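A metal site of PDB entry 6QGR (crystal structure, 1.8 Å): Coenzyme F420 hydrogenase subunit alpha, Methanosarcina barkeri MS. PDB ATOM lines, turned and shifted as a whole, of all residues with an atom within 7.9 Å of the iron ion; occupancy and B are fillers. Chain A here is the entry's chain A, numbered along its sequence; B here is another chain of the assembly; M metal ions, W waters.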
ATOM      1  N   GLU A  43     -33.973  17.632   2.043  1.00  0.00           N
ATOM      2  CA  GLU A  43     -34.592  18.716   1.261  1.00  0.00           C
ATOM      3  C   GLU A  43     -36.090  18.836   1.531  1.00  0.00           C
ATOM      4  O   GLU A  43     -36.622  19.963   1.622  1.00  0.00           O
ATOM      5  CB  GLU A  43     -34.319  18.507  -0.241  1.00  0.00           C
ATOM      6  CG  GLU A  43     -32.854  18.450  -0.528  1.00  0.00           C
ATOM      7  CD  GLU A  43     -32.544  17.664  -1.803  1.00  0.00           C
ATOM      8  OE1 GLU A  43     -33.391  16.818  -2.218  1.00  0.00           O
ATOM      9  OE2 GLU A  43     -31.473  17.934  -2.389  1.00  0.00           O
ATOM     10  N   TRP A 256     -28.017  23.839 -15.178  1.00  0.00           N
ATOM     11  CA  TRP A 256     -28.176  22.654 -14.356  1.00  0.00           C
ATOM     12  C   TRP A 256     -29.559  22.068 -14.604  1.00  0.00           C
ATOM     13  O   TRP A 256     -30.513  22.808 -14.835  1.00  0.00           O
ATOM     14  CB  TRP A 256     -27.979  23.003 -12.884  1.00  0.00           C
ATOM     15  CG  TRP A 256     -28.715  22.107 -12.018  1.00  0.00           C
ATOM     16  CD1 TRP A 256     -28.479  20.784 -11.809  1.00  0.00           C
ATOM     17  CD2 TRP A 256     -29.851  22.463 -11.206  1.00  0.00           C
ATOM     18  NE1 TRP A 256     -29.429  20.276 -10.919  1.00  0.00           N
ATOM     19  CE2 TRP A 256     -30.266  21.293 -10.536  1.00  0.00           C
ATOM     20  CE3 TRP A 256     -30.542  23.657 -10.998  1.00  0.00           C
ATOM     21  CZ2 TRP A 256     -31.357  21.267  -9.666  1.00  0.00           C
ATOM     22  CZ3 TRP A 256     -31.662  23.639 -10.118  1.00  0.00           C
ATOM     23  CH2 TRP A 256     -32.061  22.448  -9.484  1.00  0.00           C
ATOM     24  N   GLU A 258     -31.631  18.300 -12.885  1.00  0.00           N
ATOM     25  CA  GLU A 258     -31.517  17.062 -12.131  1.00  0.00           C
ATOM     26  C   GLU A 258     -32.601  16.105 -12.590  1.00  0.00           C
ATOM     27  O   GLU A 258     -33.777  16.470 -12.649  1.00  0.00           O
ATOM     28  CB  GLU A 258     -31.576  17.281 -10.611  1.00  0.00           C
ATOM     29  CG  GLU A 258     -31.040  16.014  -9.805  1.00  0.00           C
ATOM     30  CD  GLU A 258     -30.868  16.235  -8.298  1.00  0.00           C
ATOM     31  OE1 GLU A 258     -31.464  17.212  -7.794  1.00  0.00           O
ATOM     32  OE2 GLU A 258     -30.144  15.448  -7.601  1.00  0.00           O
ATOM     33  N   THR A 298     -29.774   8.135  -5.264  1.00  0.00           N
ATOM     34  CA  THR A 298     -29.543   9.562  -5.484  1.00  0.00           C
ATOM     35  C   THR A 298     -30.375  10.101  -6.652  1.00  0.00           C
ATOM     36  O   THR A 298     -30.959   9.355  -7.428  1.00  0.00           O
ATOM     37  CB  THR A 298     -28.046   9.822  -5.701  1.00  0.00           C
ATOM     38  OG1 THR A 298     -27.562   9.001  -6.772  1.00  0.00           O
ATOM     39  CG2 THR A 298     -27.236   9.487  -4.433  1.00  0.00           C
ATOM     40  N   GLY A 299     -30.452  11.451  -6.755  1.00  0.00           N
ATOM     41  CA  GLY A 299     -30.824  12.066  -8.031  1.00  0.00           C
ATOM     42  C   GLY A 299     -29.564  12.222  -8.860  1.00  0.00           C
ATOM     43  O   GLY A 299     -28.472  11.947  -8.387  1.00  0.00           O
ATOM     44  N   VAL A 300     -29.713  12.602 -10.127  1.00  0.00           N
ATOM     45  CA  VAL A 300     -28.560  12.797 -10.989  1.00  0.00           C
ATOM     46  C   VAL A 300     -28.558  14.242 -11.477  1.00  0.00           C
ATOM     47  O   VAL A 300     -29.237  14.577 -12.442  1.00  0.00           O
ATOM     48  CB  VAL A 300     -28.543  11.823 -12.182  1.00  0.00           C
ATOM     49  CG1 VAL A 300     -27.308  12.112 -13.066  1.00  0.00           C
ATOM     50  CG2 VAL A 300     -28.619  10.350 -11.717  1.00  0.00           C
ATOM     51  N   PRO A 301     -27.791  15.116 -10.853  1.00  0.00           N
ATOM     52  CA  PRO A 301     -27.615  16.452 -11.427  1.00  0.00           C
ATOM     53  C   PRO A 301     -26.730  16.384 -12.668  1.00  0.00           C
ATOM     54  O   PRO A 301     -25.783  15.593 -12.750  1.00  0.00           O
ATOM     55  CB  PRO A 301     -26.949  17.263 -10.297  1.00  0.00           C
ATOM     56  CG  PRO A 301     -26.225  16.203  -9.471  1.00  0.00           C
ATOM     57  CD  PRO A 301     -27.044  14.927  -9.598  1.00  0.00           C
ATOM     58  N   ILE A 383     -23.721  22.692  -3.868  1.00  0.00           N
ATOM     59  CA  ILE A 383     -24.614  23.797  -4.215  1.00  0.00           C
ATOM     60  C   ILE A 383     -25.939  23.570  -3.512  1.00  0.00           C
ATOM     61  O   ILE A 383     -26.590  22.524  -3.708  1.00  0.00           O
ATOM     62  CB  ILE A 383     -24.792  23.936  -5.728  1.00  0.00           C
ATOM     63  CG1 ILE A 383     -23.420  24.208  -6.379  1.00  0.00           C
ATOM     64  CG2 ILE A 383     -25.738  25.106  -6.069  1.00  0.00           C
ATOM     65  CD1 ILE A 383     -23.299  23.424  -7.580  1.00  0.00           C
ATOM     66  N   LEU A 385     -29.657  25.549  -2.727  1.00  0.00           N
ATOM     67  CA  LEU A 385     -30.550  26.554  -3.305  1.00  0.00           C
ATOM     68  C   LEU A 385     -31.774  26.662  -2.379  1.00  0.00           C
ATOM     69  O   LEU A 385     -32.256  25.646  -1.861  1.00  0.00           O
ATOM     70  CB  LEU A 385     -31.002  26.183  -4.763  1.00  0.00           C
ATOM     71  CG  LEU A 385     -29.906  25.800  -5.783  1.00  0.00           C
ATOM     72  CD1 LEU A 385     -29.600  24.301  -5.807  1.00  0.00           C
ATOM     73  CD2 LEU A 385     -30.230  26.280  -7.198  1.00  0.00           C
ATOM     74  N   TYR A 396     -36.210  24.078  -0.934  1.00  0.00           N
ATOM     75  CA  TYR A 396     -34.815  23.771  -0.611  1.00  0.00           C
ATOM     76  C   TYR A 396     -34.287  22.695  -1.553  1.00  0.00           C
ATOM     77  O   TYR A 396     -34.993  21.726  -1.851  1.00  0.00           O
ATOM     78  CB  TYR A 396     -34.680  23.298   0.842  1.00  0.00           C
ATOM     79  CG  TYR A 396     -33.269  23.463   1.372  1.00  0.00           C
ATOM     80  CD1 TYR A 396     -32.595  24.693   1.278  1.00  0.00           C
ATOM     81  CD2 TYR A 396     -32.613  22.411   1.964  1.00  0.00           C
ATOM     82  CE1 TYR A 396     -31.250  24.821   1.767  1.00  0.00           C
ATOM     83  CE2 TYR A 396     -31.308  22.548   2.463  1.00  0.00           C
ATOM     84  CZ  TYR A 396     -30.636  23.760   2.356  1.00  0.00           C
ATOM     85  OH  TYR A 396     -29.364  23.861   2.888  1.00  0.00           O
ATOM     86  N   ASP A 397     -33.046  22.829  -1.996  1.00  0.00           N
ATOM     87  CA  ASP A 397     -32.487  21.826  -2.901  1.00  0.00           C
ATOM     88  C   ASP A 397     -30.987  21.752  -2.697  1.00  0.00           C
ATOM     89  O   ASP A 397     -30.348  22.781  -2.514  1.00  0.00           O
ATOM     90  CB  ASP A 397     -32.755  22.126  -4.386  1.00  0.00           C
ATOM     91  CG  ASP A 397     -32.895  20.846  -5.247  1.00  0.00           C
ATOM     92  OD1 ASP A 397     -32.877  19.710  -4.705  1.00  0.00           O
ATOM     93  OD2 ASP A 397     -33.084  20.975  -6.459  1.00  0.00           O
ATOM     94  N   MET A 398     -30.437  20.524  -2.783  1.00  0.00           N
ATOM     95  CA  MET A 398     -29.027  20.261  -2.483  1.00  0.00           C
ATOM     96  C   MET A 398     -28.406  19.421  -3.603  1.00  0.00           C
ATOM     97  O   MET A 398     -28.868  18.301  -3.881  1.00  0.00           O
ATOM     98  CB  MET A 398     -28.886  19.554  -1.148  1.00  0.00           C
ATOM     99  CG  MET A 398     -29.211  20.403   0.050  1.00  0.00           C
ATOM    100  SD  MET A 398     -29.408  19.372   1.520  1.00  0.00           S
ATOM    101  CE  MET A 398     -27.763  18.595   1.734  1.00  0.00           C
ATOM    102  N   LEU A 399     -27.392  19.980  -4.277  1.00  0.00           N
ATOM    103  CA  LEU A 399     -26.608  19.284  -5.307  1.00  0.00           C
ATOM    104  C   LEU A 399     -25.184  19.069  -4.762  1.00  0.00           C
ATOM    105  O   LEU A 399     -24.330  19.962  -4.858  1.00  0.00           O
ATOM    106  CB  LEU A 399     -26.585  20.088  -6.619  1.00  0.00           C
ATOM    107  CG  LEU A 399     -27.877  20.836  -6.989  1.00  0.00           C
ATOM    108  CD1 LEU A 399     -27.683  21.769  -8.216  1.00  0.00           C
ATOM    109  CD2 LEU A 399     -28.996  19.844  -7.200  1.00  0.00           C
ATOM    110  N   VAL A 400     -24.919  17.885  -4.221  1.00  0.00           N
ATOM    111  CA  VAL A 400     -23.756  17.591  -3.383  1.00  0.00           C
ATOM    112  C   VAL A 400     -22.672  16.903  -4.232  1.00  0.00           C
ATOM    113  O   VAL A 400     -22.991  16.156  -5.170  1.00  0.00           O
ATOM    114  CB  VAL A 400     -24.188  16.764  -2.154  1.00  0.00           C
ATOM    115  CG1 VAL A 400     -23.075  16.567  -1.078  1.00  0.00           C
ATOM    116  CG2 VAL A 400     -25.406  17.402  -1.491  1.00  0.00           C
ATOM    117  N   THR A 403     -22.994  13.316  -5.214  1.00  0.00           N
ATOM    118  CA  THR A 403     -24.143  13.170  -6.108  1.00  0.00           C
ATOM    119  C   THR A 403     -23.735  13.386  -7.573  1.00  0.00           C
ATOM    120  O   THR A 403     -24.116  12.613  -8.468  1.00  0.00           O
ATOM    121  CB  THR A 403     -25.266  14.173  -5.746  1.00  0.00           C
ATOM    122  OG1 THR A 403     -25.383  14.361  -4.317  1.00  0.00           O
ATOM    123  CG2 THR A 403     -26.602  13.723  -6.306  1.00  0.00           C
ATOM    124  N   CYS A 434     -23.320  12.109   2.001  1.00  0.00           N
ATOM    125  CA  CYS A 434     -23.470  13.374   1.271  1.00  0.00           C
ATOM    126  C   CYS A 434     -24.289  13.242  -0.003  1.00  0.00           C
ATOM    127  O   CYS A 434     -25.208  14.027  -0.250  1.00  0.00           O
ATOM    128  CB  CYS A 434     -22.105  13.927   0.870  1.00  0.00           C
ATOM    129  SG  CYS A 434     -21.525  14.980   2.120  1.00  0.00           S
ATOM    130  N   ALA A 435     -23.946  12.276  -0.860  1.00  0.00           N
ATOM    131  CA  ALA A 435     -24.587  12.202  -2.160  1.00  0.00           C
ATOM    132  C   ALA A 435     -26.100  11.996  -2.036  1.00  0.00           C
ATOM    133  O   ALA A 435     -26.857  12.405  -2.918  1.00  0.00           O
ATOM    134  CB  ALA A 435     -23.972  11.059  -2.975  1.00  0.00           C
ATOM    135  N   THR A 436     -26.537  11.342  -0.953  1.00  0.00           N
ATOM    136  CA  THR A 436     -27.917  10.900  -0.777  1.00  0.00           C
ATOM    137  C   THR A 436     -28.751  11.908   0.017  1.00  0.00           C
ATOM    138  O   THR A 436     -29.876  12.219  -0.393  1.00  0.00           O
ATOM    139  CB  THR A 436     -27.956   9.495  -0.091  1.00  0.00           C
ATOM    140  OG1 THR A 436     -27.130   8.574  -0.828  1.00  0.00           O
ATOM    141  CG2 THR A 436     -29.341   8.905  -0.087  1.00  0.00           C
ATOM    142  N   HIS A 437     -28.206  12.391   1.148  1.00  0.00           N
ATOM    143  CA  HIS A 437     -28.851  13.346   2.052  1.00  0.00           C
ATOM    144  C   HIS A 437     -30.356  13.121   2.206  1.00  0.00           C
ATOM    145  O   HIS A 437     -30.778  12.007   2.464  1.00  0.00           O
ATOM    146  CB  HIS A 437     -28.563  14.811   1.615  1.00  0.00           C
ATOM    147  CG  HIS A 437     -28.654  15.067   0.146  1.00  0.00           C
ATOM    148  ND1 HIS A 437     -27.606  14.824  -0.727  1.00  0.00           N
ATOM    149  CD2 HIS A 437     -29.639  15.629  -0.600  1.00  0.00           C
ATOM    150  CE1 HIS A 437     -27.958  15.190  -1.955  1.00  0.00           C
ATOM    151  NE2 HIS A 437     -29.174  15.689  -1.899  1.00  0.00           N
ATOM    152  N   GLN B 103     -38.509  12.329  -1.098  1.00  0.00           N
ATOM    153  CA  GLN B 103     -37.342  12.841  -1.831  1.00  0.00           C
ATOM    154  C   GLN B 103     -36.804  11.780  -2.805  1.00  0.00           C
ATOM    155  O   GLN B 103     -36.820  10.586  -2.490  1.00  0.00           O
ATOM    156  CB  GLN B 103     -36.258  13.241  -0.835  1.00  0.00           C
ATOM    157  CG  GLN B 103     -35.034  13.860  -1.460  1.00  0.00           C
ATOM    158  CD  GLN B 103     -34.108  14.421  -0.385  1.00  0.00           C
ATOM    159  OE1 GLN B 103     -34.533  15.217   0.478  1.00  0.00           O
ATOM    160  NE2 GLN B 103     -32.843  13.984  -0.421  1.00  0.00           N
ATOM    161  N   HIS B 104     -36.318  12.205  -3.967  1.00  0.00           N
ATOM    162  CA  HIS B 104     -35.749  11.214  -4.891  1.00  0.00           C
ATOM    163  C   HIS B 104     -34.460  10.629  -4.299  1.00  0.00           C
ATOM    164  O   HIS B 104     -33.764  11.294  -3.526  1.00  0.00           O
ATOM    165  CB  HIS B 104     -35.490  11.830  -6.275  1.00  0.00           C
ATOM    166  CG  HIS B 104     -34.611  13.059  -6.288  1.00  0.00           C
ATOM    167  ND1 HIS B 104     -34.669  14.010  -7.295  1.00  0.00           N
ATOM    168  CD2 HIS B 104     -33.613  13.462  -5.455  1.00  0.00           C
ATOM    169  CE1 HIS B 104     -33.766  14.957  -7.062  1.00  0.00           C
ATOM    170  NE2 HIS B 104     -33.102  14.636  -5.968  1.00  0.00           N
HETATM  171 FE    FE M   1     -30.297  16.746  -3.713  1.00  0.00          FE
HETATM  172  O   HOH W   1     -31.495  17.461  -5.308  1.00  0.00           O
HETATM  173  O   HOH W   2     -29.339  15.466  -5.170  1.00  0.00           O
HETATM  174  O   HOH W   3     -31.972  15.099  -3.641  1.00  0.00           O
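Water W1 lies within hydrogen-bond range of the side-chain carboxylate (OE1) of Glu 258 (2.5 Å), the side-chain carboxylate (OD1) of Asp 397 (2.7 Å) and a ring nitrogen (NE2) of His 104 of chain B (3.3 Å).
Water W3 bridges a ring nitrogen (NE2) of His 104 of chain B (2.6 Å) and the side-chain carboxylate of Glu 43 (2.6 Å).
The backbone carbonyl oxygen (O) of Cys 434 lies within hydrogen-bond range of a ring nitrogen (ND1) of His 437 (2.6 Å).
N of Glu 43 is in hydrogen-bond range of OE1 of Gln 103 of chain B.
ND1 of His 437 lies close to O of Ala 435, 3.3 Å away.
The iron ion is bound by O of Met 398, 2.1 Å away.
Water W1 is bound to the iron ion, at 2.1 Å.
The iron ion is bound by OE2 of Glu 43 (2.1 Å).
Water W2 binds the iron ion (2.2 Å).
The iron ion is bound by water W3 (2.4 Å).
A ring nitrogen (NE2) of His 437 binds the iron ion.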
